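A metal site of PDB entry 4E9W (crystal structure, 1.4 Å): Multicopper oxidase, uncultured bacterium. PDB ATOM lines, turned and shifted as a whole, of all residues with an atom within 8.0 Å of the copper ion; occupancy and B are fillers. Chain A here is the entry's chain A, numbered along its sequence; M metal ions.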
ATOM      1  N   ILE A  10      17.927 -14.291 -23.037  1.00  0.00           N
ATOM      2  CA  ILE A  10      19.318 -14.700 -22.905  1.00  0.00           C
ATOM      3  C   ILE A  10      19.660 -15.410 -24.218  1.00  0.00           C
ATOM      4  O   ILE A  10      18.913 -16.338 -24.566  1.00  0.00           O
ATOM      5  CB  ILE A  10      19.595 -15.622 -21.709  1.00  0.00           C
ATOM      6  CG1 ILE A  10      18.857 -15.176 -20.437  1.00  0.00           C
ATOM      7  CG2 ILE A  10      21.093 -15.766 -21.410  1.00  0.00           C
ATOM      8  CD1 ILE A  10      19.076 -16.116 -19.271  1.00  0.00           C
ATOM      9  N   PHE A  26      26.970 -15.419 -23.433  1.00  0.00           N
ATOM     10  CA  PHE A  26      25.545 -15.565 -23.183  1.00  0.00           C
ATOM     11  C   PHE A  26      24.995 -14.156 -22.898  1.00  0.00           C
ATOM     12  O   PHE A  26      24.959 -13.728 -21.762  1.00  0.00           O
ATOM     13  CB  PHE A  26      25.272 -16.513 -22.029  1.00  0.00           C
ATOM     14  CG  PHE A  26      25.689 -17.950 -22.270  1.00  0.00           C
ATOM     15  CD1 PHE A  26      25.160 -18.686 -23.316  1.00  0.00           C
ATOM     16  CD2 PHE A  26      26.620 -18.553 -21.417  1.00  0.00           C
ATOM     17  CE1 PHE A  26      25.521 -20.008 -23.551  1.00  0.00           C
ATOM     18  CE2 PHE A  26      26.970 -19.883 -21.614  1.00  0.00           C
ATOM     19  CZ  PHE A  26      26.400 -20.604 -22.661  1.00  0.00           C
ATOM     20  N   PHE A  28      22.620 -11.061 -22.402  1.00  0.00           N
ATOM     21  CA  PHE A  28      21.256 -10.622 -22.127  1.00  0.00           C
ATOM     22  C   PHE A  28      20.811  -9.761 -23.305  1.00  0.00           C
ATOM     23  O   PHE A  28      21.529  -8.841 -23.680  1.00  0.00           O
ATOM     24  CB  PHE A  28      21.212  -9.828 -20.818  1.00  0.00           C
ATOM     25  CG  PHE A  28      21.426 -10.741 -19.616  1.00  0.00           C
ATOM     26  CD1 PHE A  28      20.505 -11.751 -19.331  1.00  0.00           C
ATOM     27  CD2 PHE A  28      22.530 -10.582 -18.791  1.00  0.00           C
ATOM     28  CE1 PHE A  28      20.679 -12.586 -18.251  1.00  0.00           C
ATOM     29  CE2 PHE A  28      22.696 -11.397 -17.688  1.00  0.00           C
ATOM     30  CZ  PHE A  28      21.763 -12.399 -17.405  1.00  0.00           C
ATOM     31  N   ASN A  51      15.060 -17.881 -21.537  1.00  0.00           N
ATOM     32  CA  ASN A  51      16.369 -18.460 -21.811  1.00  0.00           C
ATOM     33  C   ASN A  51      16.414 -19.088 -23.206  1.00  0.00           C
ATOM     34  O   ASN A  51      15.937 -20.223 -23.371  1.00  0.00           O
ATOM     35  CB  ASN A  51      16.639 -19.552 -20.759  1.00  0.00           C
ATOM     36  CG  ASN A  51      18.025 -20.124 -20.912  1.00  0.00           C
ATOM     37  OD1 ASN A  51      18.760 -19.751 -21.843  1.00  0.00           O
ATOM     38  ND2 ASN A  51      18.387 -21.013 -20.004  1.00  0.00           N
ATOM     39  N   THR A  53      19.139 -19.983 -24.728  1.00  0.00           N
ATOM     40  CA  THR A  53      20.432 -20.644 -24.909  1.00  0.00           C
ATOM     41  C   THR A  53      20.287 -22.122 -24.571  1.00  0.00           C
ATOM     42  O   THR A  53      19.218 -22.589 -24.173  1.00  0.00           O
ATOM     43  CB  THR A  53      21.540 -20.048 -24.029  1.00  0.00           C
ATOM     44  OG1 THR A  53      21.371 -20.549 -22.665  1.00  0.00           O
ATOM     45  CG2 THR A  53      21.417 -18.548 -23.940  1.00  0.00           C
ATOM     46  N   LEU A  55      21.906 -23.717 -22.158  1.00  0.00           N
ATOM     47  CA  LEU A  55      22.348 -24.027 -20.798  1.00  0.00           C
ATOM     48  C   LEU A  55      21.478 -23.274 -19.809  1.00  0.00           C
ATOM     49  O   LEU A  55      20.907 -22.243 -20.185  1.00  0.00           O
ATOM     50  CB  LEU A  55      23.793 -23.600 -20.561  1.00  0.00           C
ATOM     51  CG  LEU A  55      24.917 -24.329 -21.307  1.00  0.00           C
ATOM     52  CD1 LEU A  55      26.286 -23.754 -21.013  1.00  0.00           C
ATOM     53  CD2 LEU A  55      24.896 -25.813 -20.922  1.00  0.00           C
ATOM     54  N   PRO A  56      21.401 -23.757 -18.574  1.00  0.00           N
ATOM     55  CA  PRO A  56      20.639 -23.094 -17.514  1.00  0.00           C
ATOM     56  C   PRO A  56      21.340 -21.826 -17.013  1.00  0.00           C
ATOM     57  O   PRO A  56      22.570 -21.709 -17.007  1.00  0.00           O
ATOM     58  CB  PRO A  56      20.563 -24.116 -16.402  1.00  0.00           C
ATOM     59  CG  PRO A  56      21.614 -25.126 -16.709  1.00  0.00           C
ATOM     60  CD  PRO A  56      22.016 -25.025 -18.146  1.00  0.00           C
ATOM     61  N   HIS A  57      20.477 -20.882 -16.614  1.00  0.00           N
ATOM     62  CA  HIS A  57      20.887 -19.594 -16.067  1.00  0.00           C
ATOM     63  C   HIS A  57      19.891 -19.154 -14.992  1.00  0.00           C
ATOM     64  O   HIS A  57      18.814 -19.742 -14.859  1.00  0.00           O
ATOM     65  CB  HIS A  57      20.954 -18.530 -17.167  1.00  0.00           C
ATOM     66  CG  HIS A  57      21.806 -18.884 -18.361  1.00  0.00           C
ATOM     67  ND1 HIS A  57      23.180 -18.833 -18.360  1.00  0.00           N
ATOM     68  CD2 HIS A  57      21.456 -19.296 -19.611  1.00  0.00           C
ATOM     69  CE1 HIS A  57      23.654 -19.192 -19.537  1.00  0.00           C
ATOM     70  NE2 HIS A  57      22.612 -19.482 -20.321  1.00  0.00           N
ATOM     71  N   THR A  58      20.233 -18.092 -14.286  1.00  0.00           N
ATOM     72  CA  THR A  58      19.334 -17.309 -13.459  1.00  0.00           C
ATOM     73  C   THR A  58      19.694 -15.822 -13.643  1.00  0.00           C
ATOM     74  O   THR A  58      20.675 -15.530 -14.331  1.00  0.00           O
ATOM     75  CB  THR A  58      19.417 -17.603 -11.962  1.00  0.00           C
ATOM     76  OG1 THR A  58      20.763 -17.318 -11.514  1.00  0.00           O
ATOM     77  CG2 THR A  58      19.117 -19.071 -11.612  1.00  0.00           C
ATOM     78  N   ILE A  59      18.958 -14.927 -13.022  1.00  0.00           N
ATOM     79  CA  ILE A  59      19.453 -13.558 -12.885  1.00  0.00           C
ATOM     80  C   ILE A  59      19.347 -13.202 -11.396  1.00  0.00           C
ATOM     81  O   ILE A  59      18.276 -13.281 -10.828  1.00  0.00           O
ATOM     82  CB  ILE A  59      18.702 -12.515 -13.714  1.00  0.00           C
ATOM     83  CG1 ILE A  59      18.568 -12.836 -15.207  1.00  0.00           C
ATOM     84  CG2 ILE A  59      19.339 -11.123 -13.531  1.00  0.00           C
ATOM     85  CD1 ILE A  59      17.907 -11.685 -15.961  1.00  0.00           C
ATOM     86  N   ILE A  83      16.858 -21.547 -14.454  1.00  0.00           N
ATOM     87  CA  ILE A  83      16.020 -21.405 -15.639  1.00  0.00           C
ATOM     88  C   ILE A  83      16.638 -22.274 -16.729  1.00  0.00           C
ATOM     89  O   ILE A  83      17.689 -21.942 -17.272  1.00  0.00           O
ATOM     90  CB  ILE A  83      15.948 -19.937 -16.089  1.00  0.00           C
ATOM     91  CG1 ILE A  83      15.610 -18.993 -14.930  1.00  0.00           C
ATOM     92  CG2 ILE A  83      14.993 -19.806 -17.273  1.00  0.00           C
ATOM     93  CD1 ILE A  83      15.646 -17.505 -15.247  1.00  0.00           C
ATOM     94  N   HIS A 104      23.378 -10.106 -12.788  1.00  0.00           N
ATOM     95  CA  HIS A 104      24.260 -11.060 -13.443  1.00  0.00           C
ATOM     96  C   HIS A 104      23.729 -12.466 -13.241  1.00  0.00           C
ATOM     97  O   HIS A 104      22.959 -12.712 -12.281  1.00  0.00           O
ATOM     98  CB  HIS A 104      25.693 -10.971 -12.940  1.00  0.00           C
ATOM     99  CG  HIS A 104      25.927 -11.126 -11.466  1.00  0.00           C
ATOM    100  ND1 HIS A 104      25.956 -12.347 -10.831  1.00  0.00           N
ATOM    101  CD2 HIS A 104      26.146 -10.202 -10.484  1.00  0.00           C
ATOM    102  CE1 HIS A 104      26.187 -12.175  -9.526  1.00  0.00           C
ATOM    103  NE2 HIS A 104      26.309 -10.865  -9.298  1.00  0.00           N
ATOM    104  N   CYS A 105      24.143 -13.384 -14.096  1.00  0.00           N
ATOM    105  CA  CYS A 105      23.725 -14.765 -13.877  1.00  0.00           C
ATOM    106  C   CYS A 105      24.297 -15.253 -12.558  1.00  0.00           C
ATOM    107  O   CYS A 105      25.338 -14.740 -12.148  1.00  0.00           O
ATOM    108  CB  CYS A 105      24.228 -15.621 -15.035  1.00  0.00           C
ATOM    109  SG  CYS A 105      23.745 -17.357 -14.904  1.00  0.00           S
ATOM    110  N   HIS A 106      23.676 -16.246 -11.921  1.00  0.00           N
ATOM    111  CA  HIS A 106      24.216 -16.807 -10.688  1.00  0.00           C
ATOM    112  C   HIS A 106      24.339 -18.336 -10.778  1.00  0.00           C
ATOM    113  O   HIS A 106      24.463 -19.025  -9.766  1.00  0.00           O
ATOM    114  CB  HIS A 106      23.395 -16.421  -9.452  1.00  0.00           C
ATOM    115  CG  HIS A 106      24.210 -16.061  -8.250  1.00  0.00           C
ATOM    116  ND1 HIS A 106      24.884 -17.006  -7.508  1.00  0.00           N
ATOM    117  CD2 HIS A 106      24.458 -14.848  -7.679  1.00  0.00           C
ATOM    118  CE1 HIS A 106      25.512 -16.382  -6.525  1.00  0.00           C
ATOM    119  NE2 HIS A 106      25.272 -15.083  -6.603  1.00  0.00           N
ATOM    120  N   VAL A 107      24.325 -18.850 -11.997  1.00  0.00           N
ATOM    121  CA  VAL A 107      24.630 -20.230 -12.322  1.00  0.00           C
ATOM    122  C   VAL A 107      26.067 -20.281 -12.890  1.00  0.00           C
ATOM    123  O   VAL A 107      26.380 -19.453 -13.771  1.00  0.00           O
ATOM    124  CB  VAL A 107      23.693 -20.814 -13.381  1.00  0.00           C
ATOM    125  CG1 VAL A 107      24.166 -22.226 -13.716  1.00  0.00           C
ATOM    126  CG2 VAL A 107      22.255 -20.821 -12.927  1.00  0.00           C
ATOM    127  N   ASN A 108      26.872 -21.210 -12.411  1.00  0.00           N
ATOM    128  CA  ASN A 108      28.196 -21.420 -13.007  1.00  0.00           C
ATOM    129  C   ASN A 108      28.977 -20.123 -13.136  1.00  0.00           C
ATOM    130  O   ASN A 108      29.572 -19.812 -14.174  1.00  0.00           O
ATOM    131  CB  ASN A 108      27.983 -22.113 -14.367  1.00  0.00           C
ATOM    132  CG  ASN A 108      27.718 -23.618 -14.318  1.00  0.00           C
ATOM    133  OD1 ASN A 108      28.002 -24.302 -13.334  1.00  0.00           O
ATOM    134  ND2 ASN A 108      27.176 -24.232 -15.385  1.00  0.00           N
ATOM    135  N   VAL A 109      28.927 -19.301 -12.098  1.00  0.00           N
ATOM    136  CA  VAL A 109      29.340 -17.899 -12.158  1.00  0.00           C
ATOM    137  C   VAL A 109      30.796 -17.688 -12.599  1.00  0.00           C
ATOM    138  O   VAL A 109      31.057 -16.705 -13.295  1.00  0.00           O
ATOM    139  CB  VAL A 109      29.123 -17.136 -10.837  1.00  0.00           C
ATOM    140  CG1 VAL A 109      27.677 -17.341 -10.376  1.00  0.00           C
ATOM    141  CG2 VAL A 109      30.070 -17.511  -9.718  1.00  0.00           C
ATOM    142  N   GLU A 111      32.367 -19.109 -14.772  1.00  0.00           N
ATOM    143  CA  GLU A 111      32.397 -19.026 -16.227  1.00  0.00           C
ATOM    144  C   GLU A 111      31.422 -17.998 -16.770  1.00  0.00           C
ATOM    145  O   GLU A 111      31.784 -17.131 -17.599  1.00  0.00           O
ATOM    146  CB  GLU A 111      32.075 -20.388 -16.878  1.00  0.00           C
ATOM    147  CG  GLU A 111      32.196 -20.325 -18.394  1.00  0.00           C
ATOM    148  CD  GLU A 111      31.554 -21.470 -19.137  1.00  0.00           C
ATOM    149  OE1 GLU A 111      31.201 -22.491 -18.496  1.00  0.00           O
ATOM    150  OE2 GLU A 111      31.442 -21.294 -20.393  1.00  0.00           O
ATOM    151  N   HIS A 112      30.157 -18.080 -16.322  1.00  0.00           N
ATOM    152  CA  HIS A 112      29.125 -17.250 -16.979  1.00  0.00           C
ATOM    153  C   HIS A 112      29.368 -15.759 -16.744  1.00  0.00           C
ATOM    154  O   HIS A 112      29.204 -14.933 -17.651  1.00  0.00           O
ATOM    155  CB  HIS A 112      27.737 -17.692 -16.494  1.00  0.00           C
ATOM    156  CG  HIS A 112      27.327 -19.028 -17.072  1.00  0.00           C
ATOM    157  ND1 HIS A 112      26.007 -19.438 -17.137  1.00  0.00           N
ATOM    158  CD2 HIS A 112      28.077 -20.034 -17.589  1.00  0.00           C
ATOM    159  CE1 HIS A 112      25.961 -20.642 -17.680  1.00  0.00           C
ATOM    160  NE2 HIS A 112      27.201 -21.028 -17.971  1.00  0.00           N
ATOM    161  N   VAL A 113      29.762 -15.440 -15.501  1.00  0.00           N
ATOM    162  CA  VAL A 113      30.001 -14.038 -15.171  1.00  0.00           C
ATOM    163  C   VAL A 113      31.434 -13.726 -15.500  1.00  0.00           C
ATOM    164  O   VAL A 113      31.743 -12.646 -16.011  1.00  0.00           O
ATOM    165  CB  VAL A 113      29.683 -13.691 -13.698  1.00  0.00           C
ATOM    166  CG1 VAL A 113      29.979 -12.224 -13.419  1.00  0.00           C
ATOM    167  CG2 VAL A 113      28.223 -14.037 -13.388  1.00  0.00           C
ATOM    168  N   ARG A 116      31.524 -15.040 -19.853  1.00  0.00           N
ATOM    169  CA  ARG A 116      30.457 -15.149 -20.863  1.00  0.00           C
ATOM    170  C   ARG A 116      29.550 -13.923 -20.860  1.00  0.00           C
ATOM    171  O   ARG A 116      28.477 -13.923 -21.466  1.00  0.00           O
ATOM    172  CB  ARG A 116      29.632 -16.413 -20.646  1.00  0.00           C
ATOM    173  CG  ARG A 116      30.424 -17.709 -20.780  1.00  0.00           C
ATOM    174  CD  ARG A 116      31.060 -17.964 -22.134  1.00  0.00           C
ATOM    175  NE  ARG A 116      32.043 -19.056 -22.034  1.00  0.00           N
ATOM    176  CZ  ARG A 116      33.032 -19.287 -22.878  1.00  0.00           C
ATOM    177  NH1 ARG A 116      33.225 -18.553 -23.956  1.00  0.00           N
ATOM    178  NH2 ARG A 116      33.823 -20.313 -22.588  1.00  0.00           N
ATOM    179  N   MET A 118      27.594 -12.345 -18.778  1.00  0.00           N
ATOM    180  CA  MET A 118      26.228 -12.351 -18.240  1.00  0.00           C
ATOM    181  C   MET A 118      26.028 -11.323 -17.139  1.00  0.00           C
ATOM    182  O   MET A 118      25.870 -11.652 -15.954  1.00  0.00           O
ATOM    183  CB  MET A 118      25.910 -13.769 -17.745  1.00  0.00           C
ATOM    184  CG  MET A 118      26.119 -14.825 -18.857  1.00  0.00           C
ATOM    185  SD  MET A 118      25.027 -16.244 -18.534  1.00  0.00           S
ATOM    186  CE  MET A 118      23.391 -15.538 -18.811  1.00  0.00           C
HETATM  187 CU    CU M   1      24.398 -18.274 -16.795  1.00  0.00          CU
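The copper ion is bound by a ring nitrogen (ND1) of His 112 (2.0 Å), a ring nitrogen (ND1) of His 57 (2.1 Å), the side-chain sulfur of Cys 105 (2.2 Å) and the side-chain sulfur of Met 118 (2.7 Å). The copper ion has four donor atoms within binding distance.
Residues that only touch the copper ion: Pro 56 (3.9 Å) and Val 107 (3.8 Å). Six residues have an atom within 4 Å of the copper ion: Pro 56, His 57, Cys 105, Val 107, His 112 and Met 118.
The side-chain hydroxyl of Thr 53 lies within hydrogen-bond range of a ring nitrogen (NE2) of His 57 (2.9 Å). The backbone carbonyl oxygen of Leu 55 sits close to a ring nitrogen (NE2) of His 57. A ring nitrogen (ND1) of His 112 lies close to the backbone carbonyl oxygen of Val 107 (3.4 Å). O of His 57 sits at hydrogen-bond distance from N of Ile 83. SG of Cys 105 lies close to O of Thr 58, 3.6 Å away. The side-chain sulfur (SG) of Cys 105 sits close to the backbone NH (N) of Val 107, at 3.3 Å.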
